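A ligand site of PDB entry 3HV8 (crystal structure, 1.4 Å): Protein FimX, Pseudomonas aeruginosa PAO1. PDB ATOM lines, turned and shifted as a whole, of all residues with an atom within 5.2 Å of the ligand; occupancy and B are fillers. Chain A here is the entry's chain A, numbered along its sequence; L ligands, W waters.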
ATOM      1  N   GLN A  38     -11.104  16.577  -9.074  1.00  0.00           N
ATOM      2  CA  GLN A  38     -11.001  15.766  -7.874  1.00  0.00           C
ATOM      3  C   GLN A  38     -11.383  14.335  -8.188  1.00  0.00           C
ATOM      4  O   GLN A  38     -12.508  14.056  -8.603  1.00  0.00           O
ATOM      5  CB  GLN A  38     -11.884  16.322  -6.746  1.00  0.00           C
ATOM      6  CG  GLN A  38     -11.718  15.520  -5.459  1.00  0.00           C
ATOM      7  CD  GLN A  38     -12.473  16.086  -4.285  1.00  0.00           C
ATOM      8  OE1 GLN A  38     -13.438  16.844  -4.448  1.00  0.00           O
ATOM      9  NE2 GLN A  38     -12.040  15.725  -3.080  1.00  0.00           N
ATOM     10  N   GLU A  52     -14.210  14.590 -10.847  1.00  0.00           N
ATOM     11  CA  GLU A  52     -15.165  15.687 -10.813  1.00  0.00           C
ATOM     12  C   GLU A  52     -14.467  16.986 -11.168  1.00  0.00           C
ATOM     13  O   GLU A  52     -13.371  17.270 -10.676  1.00  0.00           O
ATOM     14  CB  GLU A  52     -15.793  15.804  -9.416  1.00  0.00           C
ATOM     15  CG  GLU A  52     -16.832  16.902  -9.329  1.00  0.00           C
ATOM     16  CD  GLU A  52     -17.401  17.035  -7.935  1.00  0.00           C
ATOM     17  OE1 GLU A  52     -16.819  16.489  -6.966  1.00  0.00           O
ATOM     18  OE2 GLU A  52     -18.479  17.670  -7.806  1.00  0.00           O
ATOM     19  N   VAL A  53     -15.114  17.758 -12.015  1.00  0.00           N
ATOM     20  CA  VAL A  53     -14.655  19.094 -12.400  1.00  0.00           C
ATOM     21  C   VAL A  53     -15.252  20.137 -11.430  1.00  0.00           C
ATOM     22  O   VAL A  53     -16.458  20.144 -11.159  1.00  0.00           O
ATOM     23  CB  VAL A  53     -15.088  19.420 -13.830  1.00  0.00           C
ATOM     24  CG1 VAL A  53     -14.703  20.834 -14.216  1.00  0.00           C
ATOM     25  CG2 VAL A  53     -14.473  18.396 -14.811  1.00  0.00           C
ATOM     26  N   LEU A  54     -14.384  20.996 -10.896  1.00  0.00           N
ATOM     27  CA  LEU A  54     -14.800  22.066  -9.991  1.00  0.00           C
ATOM     28  C   LEU A  54     -14.254  23.389 -10.489  1.00  0.00           C
ATOM     29  O   LEU A  54     -13.083  23.486 -10.897  1.00  0.00           O
ATOM     30  CB  LEU A  54     -14.311  21.797  -8.569  1.00  0.00           C
ATOM     31  CG  LEU A  54     -14.880  20.525  -7.937  1.00  0.00           C
ATOM     32  CD1 LEU A  54     -14.078  20.102  -6.718  1.00  0.00           C
ATOM     33  CD2 LEU A  54     -16.355  20.675  -7.583  1.00  0.00           C
ATOM     34  N   LEU A  55     -15.096  24.420 -10.463  1.00  0.00           N
ATOM     35  CA  LEU A  55     -14.768  25.703 -11.082  1.00  0.00           C
ATOM     36  C   LEU A  55     -14.200  26.737 -10.106  1.00  0.00           C
ATOM     37  O   LEU A  55     -14.688  26.875  -8.995  1.00  0.00           O
ATOM     38  CB  LEU A  55     -16.039  26.306 -11.689  1.00  0.00           C
ATOM     39  CG  LEU A  55     -15.847  27.653 -12.383  1.00  0.00           C
ATOM     40  CD1 LEU A  55     -14.926  27.505 -13.585  1.00  0.00           C
ATOM     41  CD2 LEU A  55     -17.189  28.205 -12.797  1.00  0.00           C
ATOM     42  N   ARG A  56     -13.165  27.454 -10.523  1.00  0.00           N
ATOM     43  CA  ARG A  56     -12.705  28.609  -9.757  1.00  0.00           C
ATOM     44  C   ARG A  56     -12.659  29.815 -10.681  1.00  0.00           C
ATOM     45  O   ARG A  56     -12.240  29.706 -11.838  1.00  0.00           O
ATOM     46  CB  ARG A  56     -11.307  28.373  -9.186  1.00  0.00           C
ATOM     47  CG  ARG A  56     -11.182  27.161  -8.269  1.00  0.00           C
ATOM     48  CD  ARG A  56     -11.973  27.388  -6.985  1.00  0.00           C
ATOM     49  NE  ARG A  56     -11.862  26.264  -6.059  1.00  0.00           N
ATOM     50  CZ  ARG A  56     -12.783  25.306  -5.927  1.00  0.00           C
ATOM     51  NH1 ARG A  56     -13.872  25.315  -6.692  1.00  0.00           N
ATOM     52  NH2 ARG A  56     -12.594  24.324  -5.047  1.00  0.00           N
ATOM     53  N   PRO A  66     -13.754  30.848  -5.015  1.00  0.00           N
ATOM     54  CA  PRO A  66     -14.682  29.712  -5.005  1.00  0.00           C
ATOM     55  C   PRO A  66     -16.082  30.064  -5.471  1.00  0.00           C
ATOM     56  O   PRO A  66     -16.487  31.234  -5.380  1.00  0.00           O
ATOM     57  CB  PRO A  66     -14.734  29.320  -3.523  1.00  0.00           C
ATOM     58  CG  PRO A  66     -14.415  30.566  -2.788  1.00  0.00           C
ATOM     59  CD  PRO A  66     -13.523  31.397  -3.669  1.00  0.00           C
ATOM     60  N   PRO A  67     -16.825  29.063  -5.962  1.00  0.00           N
ATOM     61  CA  PRO A  67     -18.185  29.230  -6.499  1.00  0.00           C
ATOM     62  C   PRO A  67     -19.122  29.968  -5.548  1.00  0.00           C
ATOM     63  O   PRO A  67     -19.996  30.719  -6.001  1.00  0.00           O
ATOM     64  CB  PRO A  67     -18.666  27.790  -6.667  1.00  0.00           C
ATOM     65  CG  PRO A  67     -17.408  27.022  -6.937  1.00  0.00           C
ATOM     66  CD  PRO A  67     -16.323  27.690  -6.155  1.00  0.00           C
ATOM     67  N   LEU A  71     -21.309  32.268  -8.110  1.00  0.00           N
ATOM     68  CA  LEU A  71     -22.340  31.557  -8.881  1.00  0.00           C
ATOM     69  C   LEU A  71     -23.745  32.090  -8.671  1.00  0.00           C
ATOM     70  O   LEU A  71     -24.524  32.196  -9.633  1.00  0.00           O
ATOM     71  CB  LEU A  71     -22.312  30.040  -8.622  1.00  0.00           C
ATOM     72  CG  LEU A  71     -21.204  29.252  -9.312  1.00  0.00           C
ATOM     73  CD1 LEU A  71     -21.392  27.766  -8.996  1.00  0.00           C
ATOM     74  CD2 LEU A  71     -21.237  29.497 -10.811  1.00  0.00           C
ATOM     75  N   ASP A  84     -21.687  27.770 -17.442  1.00  0.00           N
ATOM     76  CA  ASP A  84     -21.773  26.339 -17.672  1.00  0.00           C
ATOM     77  C   ASP A  84     -21.208  25.953 -19.049  1.00  0.00           C
ATOM     78  O   ASP A  84     -20.514  24.955 -19.169  1.00  0.00           O
ATOM     79  CB  ASP A  84     -23.221  25.838 -17.523  1.00  0.00           C
ATOM     80  CG  ASP A  84     -23.668  25.738 -16.070  1.00  0.00           C
ATOM     81  OD1 ASP A  84     -22.823  25.795 -15.150  1.00  0.00           O
ATOM     82  OD2 ASP A  84     -24.885  25.610 -15.861  1.00  0.00           O
ATOM     83  N   VAL A  87     -17.456  25.903 -18.856  1.00  0.00           N
ATOM     84  CA  VAL A  87     -16.969  24.733 -18.152  1.00  0.00           C
ATOM     85  C   VAL A  87     -17.058  23.496 -19.038  1.00  0.00           C
ATOM     86  O   VAL A  87     -16.109  22.732 -19.131  1.00  0.00           O
ATOM     87  CB  VAL A  87     -17.753  24.492 -16.851  1.00  0.00           C
ATOM     88  CG1 VAL A  87     -17.391  23.127 -16.248  1.00  0.00           C
ATOM     89  CG2 VAL A  87     -17.490  25.636 -15.840  1.00  0.00           C
ATOM     90  N   HIS A 110     -20.796  19.757 -13.299  1.00  0.00           N
ATOM     91  CA  HIS A 110     -21.990  20.366 -12.710  1.00  0.00           C
ATOM     92  C   HIS A 110     -22.793  21.163 -13.724  1.00  0.00           C
ATOM     93  O   HIS A 110     -22.230  21.790 -14.645  1.00  0.00           O
ATOM     94  CB  HIS A 110     -21.571  21.329 -11.600  1.00  0.00           C
ATOM     95  CG  HIS A 110     -21.067  20.663 -10.365  1.00  0.00           C
ATOM     96  ND1 HIS A 110     -21.896  20.044  -9.458  1.00  0.00           N
ATOM     97  CD2 HIS A 110     -19.817  20.544  -9.867  1.00  0.00           C
ATOM     98  CE1 HIS A 110     -21.173  19.569  -8.458  1.00  0.00           C
ATOM     99  NE2 HIS A 110     -19.907  19.854  -8.693  1.00  0.00           N
ATOM    100  N   LEU A 111     -24.112  21.141 -13.547  1.00  0.00           N
ATOM    101  CA  LEU A 111     -25.012  22.057 -14.260  1.00  0.00           C
ATOM    102  C   LEU A 111     -25.767  22.920 -13.263  1.00  0.00           C
ATOM    103  O   LEU A 111     -26.327  22.409 -12.269  1.00  0.00           O
ATOM    104  CB  LEU A 111     -26.019  21.263 -15.109  1.00  0.00           C
ATOM    105  CG  LEU A 111     -25.413  20.492 -16.268  1.00  0.00           C
ATOM    106  CD1 LEU A 111     -26.535  19.727 -16.984  1.00  0.00           C
ATOM    107  CD2 LEU A 111     -24.641  21.398 -17.253  1.00  0.00           C
ATOM    108  N   SER A 112     -25.834  24.215 -13.524  1.00  0.00           N
ATOM    109  CA  SER A 112     -26.689  25.099 -12.719  1.00  0.00           C
ATOM    110  C   SER A 112     -28.160  24.912 -13.108  1.00  0.00           C
ATOM    111  O   SER A 112     -28.480  24.353 -14.157  1.00  0.00           O
ATOM    112  CB  SER A 112     -26.303  26.571 -12.933  1.00  0.00           C
ATOM    113  OG  SER A 112     -26.662  26.988 -14.235  1.00  0.00           O
ATOM    114  N   SER A 172     -26.515  14.859  -7.284  1.00  0.00           N
ATOM    115  CA  SER A 172     -25.637  15.061  -6.145  1.00  0.00           C
ATOM    116  C   SER A 172     -26.410  15.630  -4.959  1.00  0.00           C
ATOM    117  O   SER A 172     -27.574  16.019  -5.100  1.00  0.00           O
ATOM    118  CB  SER A 172     -24.496  15.994  -6.511  1.00  0.00           C
ATOM    119  OG  SER A 172     -24.972  17.263  -6.887  1.00  0.00           O
ATOM    120  N   GLN A 173     -25.755  15.670  -3.814  1.00  0.00           N
ATOM    121  CA  GLN A 173     -26.380  16.095  -2.566  1.00  0.00           C
ATOM    122  C   GLN A 173     -27.650  15.306  -2.265  1.00  0.00           C
ATOM    123  O   GLN A 173     -28.586  15.802  -1.683  1.00  0.00           O
ATOM    124  CB  GLN A 173     -26.624  17.616  -2.562  1.00  0.00           C
ATOM    125  CG  GLN A 173     -25.307  18.408  -2.597  1.00  0.00           C
ATOM    126  CD  GLN A 173     -25.482  19.886  -2.910  1.00  0.00           C
ATOM    127  OE1 GLN A 173     -26.603  20.393  -2.984  1.00  0.00           O
ATOM    128  NE2 GLN A 173     -24.373  20.586  -3.090  1.00  0.00           N
ATOM    129  N   PHE A 229     -16.837  13.470   0.753  1.00  0.00           N
ATOM    130  CA  PHE A 229     -16.389  14.000   2.048  1.00  0.00           C
ATOM    131  C   PHE A 229     -15.656  12.972   2.904  1.00  0.00           C
ATOM    132  O   PHE A 229     -15.687  13.024   4.136  1.00  0.00           O
ATOM    133  CB  PHE A 229     -17.567  14.622   2.825  1.00  0.00           C
ATOM    134  CG  PHE A 229     -17.955  16.007   2.337  1.00  0.00           C
ATOM    135  CD1 PHE A 229     -17.788  17.118   3.155  1.00  0.00           C
ATOM    136  CD2 PHE A 229     -18.468  16.195   1.071  1.00  0.00           C
ATOM    137  CE1 PHE A 229     -18.132  18.385   2.710  1.00  0.00           C
ATOM    138  CE2 PHE A 229     -18.814  17.467   0.612  1.00  0.00           C
ATOM    139  CZ  PHE A 229     -18.645  18.560   1.439  1.00  0.00           C
ATOM    140  N   VAL A 230     -14.998  12.021   2.258  1.00  0.00           N
ATOM    141  CA  VAL A 230     -14.163  11.065   2.996  1.00  0.00           C
ATOM    142  C   VAL A 230     -12.902  11.780   3.466  1.00  0.00           C
ATOM    143  O   VAL A 230     -12.068  12.188   2.656  1.00  0.00           O
ATOM    144  CB  VAL A 230     -13.824   9.831   2.135  1.00  0.00           C
ATOM    145  CG1 VAL A 230     -12.911   8.873   2.929  1.00  0.00           C
ATOM    146  CG2 VAL A 230     -15.091   9.117   1.697  1.00  0.00           C
ATOM    147  N   GLU A 231     -12.775  11.949   4.784  1.00  0.00           N
ATOM    148  CA  GLU A 231     -11.603  12.640   5.329  1.00  0.00           C
ATOM    149  C   GLU A 231     -10.838  11.793   6.335  1.00  0.00           C
ATOM    150  O   GLU A 231      -9.888  12.294   6.951  1.00  0.00           O
ATOM    151  CB  GLU A 231     -12.015  13.950   5.994  1.00  0.00           C
ATOM    152  CG  GLU A 231     -12.750  14.903   5.028  1.00  0.00           C
ATOM    153  CD  GLU A 231     -12.852  16.314   5.560  1.00  0.00           C
ATOM    154  OE1 GLU A 231     -13.836  17.008   5.241  1.00  0.00           O
ATOM    155  OE2 GLU A 231     -11.949  16.734   6.313  1.00  0.00           O
ATOM    156  N   GLN A 248     -15.058   9.665  -2.576  1.00  0.00           N
ATOM    157  CA  GLN A 248     -14.341  10.878  -2.908  1.00  0.00           C
ATOM    158  C   GLN A 248     -14.097  11.637  -1.606  1.00  0.00           C
ATOM    159  O   GLN A 248     -14.890  11.543  -0.668  1.00  0.00           O
ATOM    160  CB  GLN A 248     -15.189  11.729  -3.851  1.00  0.00           C
ATOM    161  CG  GLN A 248     -14.451  12.892  -4.480  1.00  0.00           C
ATOM    162  CD  GLN A 248     -15.402  13.895  -5.094  1.00  0.00           C
ATOM    163  OE1 GLN A 248     -16.388  14.278  -4.481  1.00  0.00           O
ATOM    164  NE2 GLN A 248     -15.101  14.324  -6.305  1.00  0.00           N
ATOM    165  N   GLY A 249     -12.999  12.394  -1.558  1.00  0.00           N
ATOM    166  CA  GLY A 249     -12.739  13.229  -0.398  1.00  0.00           C
ATOM    167  C   GLY A 249     -11.301  13.654  -0.298  1.00  0.00           C
ATOM    168  O   GLY A 249     -10.434  13.154  -1.011  1.00  0.00           O
ATOM    169  N   TYR A 250     -11.056  14.619   0.593  1.00  0.00           N
ATOM    170  CA  TYR A 250      -9.699  15.077   0.853  1.00  0.00           C
ATOM    171  C   TYR A 250      -8.753  13.940   1.239  1.00  0.00           C
ATOM    172  O   TYR A 250      -7.565  13.993   0.934  1.00  0.00           O
ATOM    173  CB  TYR A 250      -9.711  16.143   1.962  1.00  0.00           C
ATOM    174  CG  TYR A 250     -10.340  17.466   1.603  1.00  0.00           C
ATOM    175  CD1 TYR A 250     -10.923  18.276   2.580  1.00  0.00           C
ATOM    176  CD2 TYR A 250     -10.350  17.936   0.281  1.00  0.00           C
ATOM    177  CE1 TYR A 250     -11.500  19.491   2.260  1.00  0.00           C
ATOM    178  CE2 TYR A 250     -10.927  19.151  -0.039  1.00  0.00           C
ATOM    179  CZ  TYR A 250     -11.497  19.934   0.948  1.00  0.00           C
ATOM    180  OH  TYR A 250     -12.074  21.136   0.622  1.00  0.00           O
ATOM    181  N   TYR A 251      -9.279  12.917   1.916  1.00  0.00           N
ATOM    182  CA  TYR A 251      -8.459  11.771   2.342  1.00  0.00           C
ATOM    183  C   TYR A 251      -7.838  11.034   1.156  1.00  0.00           C
ATOM    184  O   TYR A 251      -6.716  10.532   1.239  1.00  0.00           O
ATOM    185  CB  TYR A 251      -9.276  10.798   3.197  1.00  0.00           C
ATOM    186  CG  TYR A 251      -8.422   9.824   3.994  1.00  0.00           C
ATOM    187  CD1 TYR A 251      -8.230   8.516   3.561  1.00  0.00           C
ATOM    188  CD2 TYR A 251      -7.819  10.212   5.187  1.00  0.00           C
ATOM    189  CE1 TYR A 251      -7.452   7.626   4.289  1.00  0.00           C
ATOM    190  CE2 TYR A 251      -7.040   9.326   5.925  1.00  0.00           C
ATOM    191  CZ  TYR A 251      -6.862   8.028   5.468  1.00  0.00           C
ATOM    192  OH  TYR A 251      -6.093   7.151   6.203  1.00  0.00           O
ATOM    193  N   PRO A 255      -9.216  18.619  -4.667  1.00  0.00           N
ATOM    194  CA  PRO A 255      -9.216  19.173  -6.025  1.00  0.00           C
ATOM    195  C   PRO A 255      -7.822  19.670  -6.416  1.00  0.00           C
ATOM    196  O   PRO A 255      -7.159  20.270  -5.578  1.00  0.00           O
ATOM    197  CB  PRO A 255     -10.186  20.350  -5.924  1.00  0.00           C
ATOM    198  CG  PRO A 255     -11.096  20.003  -4.771  1.00  0.00           C
ATOM    199  CD  PRO A 255     -10.192  19.300  -3.797  1.00  0.00           C
HETATM  200  P1  LIG L   1     -20.597  20.450  -4.267  1.00  0.00           P
HETATM  201  O1  LIG L   1     -21.471  19.126  -4.447  1.00  0.00           O
HETATM  202  O2  LIG L   1     -20.746  20.870  -2.867  1.00  0.00           O
HETATM  203  O3  LIG L   1     -19.020  20.226  -4.429  1.00  0.00           O
HETATM  204  C1  LIG L   1     -18.314  19.697  -3.285  1.00  0.00           C
HETATM  205  C2  LIG L   1     -17.626  20.792  -2.435  1.00  0.00           C
HETATM  206  O4  LIG L   1     -16.884  20.137  -1.374  1.00  0.00           O
HETATM  207  C3  LIG L   1     -16.575  21.424  -3.341  1.00  0.00           C
HETATM  208  O5  LIG L   1     -16.488  22.827  -3.046  1.00  0.00           O
HETATM  209  C4  LIG L   1     -15.273  20.649  -3.015  1.00  0.00           C
HETATM  210  O6  LIG L   1     -14.097  21.419  -3.200  1.00  0.00           O
HETATM  211  C5  LIG L   1     -15.491  20.348  -1.529  1.00  0.00           C
HETATM  212  N1  LIG L   1     -14.792  19.170  -1.043  1.00  0.00           N
HETATM  213  C6  LIG L   1     -14.254  18.145  -1.785  1.00  0.00           C
HETATM  214  N2  LIG L   1     -13.856  17.175  -0.989  1.00  0.00           N
HETATM  215  C7  LIG L   1     -14.109  17.550   0.300  1.00  0.00           C
HETATM  216  C8  LIG L   1     -13.898  16.924   1.554  1.00  0.00           C
HETATM  217  O7  LIG L   1     -13.436  15.785   1.661  1.00  0.00           O
HETATM  218  N3  LIG L   1     -14.257  17.617   2.639  1.00  0.00           N
HETATM  219  C9  LIG L   1     -14.802  18.863   2.552  1.00  0.00           C
HETATM  220  N4  LIG L   1     -15.148  19.502   3.713  1.00  0.00           N
HETATM  221  N5  LIG L   1     -15.008  19.454   1.400  1.00  0.00           N
HETATM  222  C10 LIG L   1     -14.677  18.817   0.273  1.00  0.00           C
HETATM  223  P2  LIG L   1     -16.427  23.829  -4.300  1.00  0.00           P
HETATM  224  O8  LIG L   1     -16.254  25.284  -3.732  1.00  0.00           O
HETATM  225  O9  LIG L   1     -15.409  23.402  -5.279  1.00  0.00           O
HETATM  226  O10 LIG L   1     -17.841  23.656  -4.996  1.00  0.00           O
HETATM  227  C11 LIG L   1     -19.022  24.008  -4.271  1.00  0.00           C
HETATM  228  C12 LIG L   1     -20.259  23.933  -5.180  1.00  0.00           C
HETATM  229  O11 LIG L   1     -20.098  24.861  -6.264  1.00  0.00           O
HETATM  230  C13 LIG L   1     -20.471  22.574  -5.848  1.00  0.00           C
HETATM  231  O12 LIG L   1     -21.219  21.675  -5.043  1.00  0.00           O
HETATM  232  C14 LIG L   1     -21.349  22.981  -7.030  1.00  0.00           C
HETATM  233  O13 LIG L   1     -22.696  23.233  -6.592  1.00  0.00           O
HETATM  234  C15 LIG L   1     -20.757  24.349  -7.400  1.00  0.00           C
HETATM  235  N6  LIG L   1     -19.785  24.152  -8.468  1.00  0.00           N
HETATM  236  C16 LIG L   1     -18.442  23.909  -8.365  1.00  0.00           C
HETATM  237  N7  LIG L   1     -17.949  23.814  -9.560  1.00  0.00           N
HETATM  238  C17 LIG L   1     -18.915  24.071 -10.496  1.00  0.00           C
HETATM  239  C18 LIG L   1     -18.976  24.159 -11.894  1.00  0.00           C
HETATM  240  O14 LIG L   1     -18.023  23.875 -12.631  1.00  0.00           O
HETATM  241  N8  LIG L   1     -20.189  24.466 -12.419  1.00  0.00           N
HETATM  242  C19 LIG L   1     -21.297  24.700 -11.655  1.00  0.00           C
HETATM  243  N9  LIG L   1     -22.490  24.966 -12.262  1.00  0.00           N
HETATM  244  N10 LIG L   1     -21.268  24.596 -10.343  1.00  0.00           N
HETATM  245  C20 LIG L   1     -20.098  24.306  -9.766  1.00  0.00           C
HETATM  246  O   HOH W   1     -21.296  17.214  -2.445  1.00  0.00           O
HETATM  247  O   HOH W   2     -16.735  21.838   1.401  1.00  0.00           O
HETATM  248  O   HOH W   3     -16.707  18.190   6.132  1.00  0.00           O
HETATM  249  O   HOH W   4     -13.730  23.832  -1.253  1.00  0.00           O
HETATM  250  O   HOH W   5     -23.702  19.272  -5.720  1.00  0.00           O
HETATM  251  O   HOH W   6     -11.614  21.802  -1.945  1.00  0.00           O
HETATM  252  O   HOH W   7     -20.204  17.219  -5.872  1.00  0.00           O
HETATM  253  O   HOH W   8     -20.641  24.019 -15.139  1.00  0.00           O
HETATM  254  O   HOH W   9     -16.704  21.972   4.104  1.00  0.00           O
HETATM  255  O   HOH W  10     -24.209  24.328  -9.927  1.00  0.00           O
HETATM  256  O   HOH W  11     -14.518  26.139  -2.006  1.00  0.00           O
HETATM  257  O   HOH W  12     -16.897  24.360  -0.483  1.00  0.00           O
HETATM  258  O   HOH W  13     -18.274  21.069 -12.984  1.00  0.00           O
HETATM  259  O   HOH W  14     -24.615  21.455  -6.614  1.00  0.00           O
HETATM  260  O   HOH W  15     -17.846  27.345  -2.973  1.00  0.00           O
HETATM  261  O   HOH W  16     -15.799  14.824  -1.686  1.00  0.00           O
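O of Gln 38 is in hydrogen-bond range of NE2 of Gln 248 (3.5 Å). The backbone carbonyl oxygen (O) of Val 230 sits at hydrogen-bond distance from the backbone NH (N) of Tyr 250 (3.3 Å). The side-chain carboxylate (OE2) of Glu 52 sits at hydrogen-bond distance from a ring nitrogen (NE2) of His 110 (2.8 Å). N of Val 230 lies within hydrogen-bond range of O of Gln 248 (3.0 Å). The backbone carbonyl oxygen (O) of Val 230 lies within hydrogen-bond range of the backbone NH (N) of Tyr 251 (3.0 Å). N of Phe 229 lies within hydrogen-bond range of O of Gln 248 (3.1 Å). N of Gln 38 is in hydrogen-bond range of O of Glu 52 (2.9 Å). The side-chain carboxylate of Asp 84 is in hydrogen-bond range of the side-chain hydroxyl of Ser 112.
Leu 54 touches the ligand (CA to N7, 3.6 Å). CB of Pro 67 touches O11 of the ligand, 3.3 Å away. CD1 of Leu 71 touches N10 of the ligand, 3.4 Å away. CG2 of Val 87 touches O14 of the ligand (3.7 Å). His 110 touches the ligand (CB to C19, 3.4 Å). C of Leu 111 touches N9 of the ligand, 3.99 Å away. Ser 112 touches the ligand (N to N9, 3.7 Å). Gln 173 touches the ligand. Phe 229 touches the ligand (CE1 to N4, 3.3 Å). O of Val 230 touches O7 of the ligand, 3.97 Å away. Gly 249 touches the ligand (CA to O7, 3.4 Å). CG of Pro 255 touches O6 of the ligand (3.7 Å). Hydrophobic or aromatic side chains that line the ligand: Leu 54, Leu 55, Pro 67, Leu 71, Val 87, His 110, Phe 229, Tyr 250 and Pro 255. Within 4 Å of the ligand: Gln 38, Leu 54, Leu 55, Arg 56, Pro 67, Leu 71, Asp 84, Val 87, His 110, Leu 111, Ser 112, Gln 173, Phe 229, Val 230, Glu 231, Gly 249, Tyr 250 and Pro 255.
Water W5 lies within hydrogen-bond range of an oxygen (O1) of the ligand (2.6 Å), the side-chain hydroxyl of Ser 172 (2.6 Å) and the side-chain amide nitrogen of Gln 173 (3.0 Å). Water W7 lies within hydrogen-bond range of OE2 of Glu 52 and O1 of the ligand. Water W8 lies within hydrogen-bond range of the backbone carbonyl oxygen (O) of His 110, a nitrogen (N8) of the ligand and the side-chain carboxylate (OD1) of Asp 84. Water W13 lies within hydrogen-bond range of the backbone carbonyl oxygen (O) of Val 53 (2.7 Å), an oxygen (O14) of the ligand (2.8 Å) and the backbone NH (N) of His 110 (2.9 Å). Water W16 lies within hydrogen-bond range of OE1 of Gln 248 (2.9 Å), N of Phe 229 (3.0 Å) and N2 of the ligand (3.1 Å). Water W3 bridges N4 of the ligand (3.2 Å) and OE1 of Glu 231 (3.2 Å).
An oxygen (O7) of the ligand sits at hydrogen-bond distance from the backbone NH (N) of Tyr 250 (2.9 Å). A nitrogen (N5) of the ligand lies within hydrogen-bond range of the side-chain hydroxyl of Tyr 250, at 3.5 Å. The guanidinium group (NH1) of Arg 56 is in salt-bridge range of an oxygen (O9) of the ligand (2.8 Å). OE1 of Glu 231 is in hydrogen-bond range of N3 of the ligand. A nitrogen (N9) of the ligand sits at hydrogen-bond distance from the side-chain carboxylate of Asp 84 (3.0 Å). The backbone NH (N) of Leu 55 lies within hydrogen-bond range of a nitrogen (N7) of the ligand, at 3.1 Å. The side-chain amide nitrogen (NE2) of Gln 38 is in hydrogen-bond range of a nitrogen (N2) of the ligand (3.1 Å).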
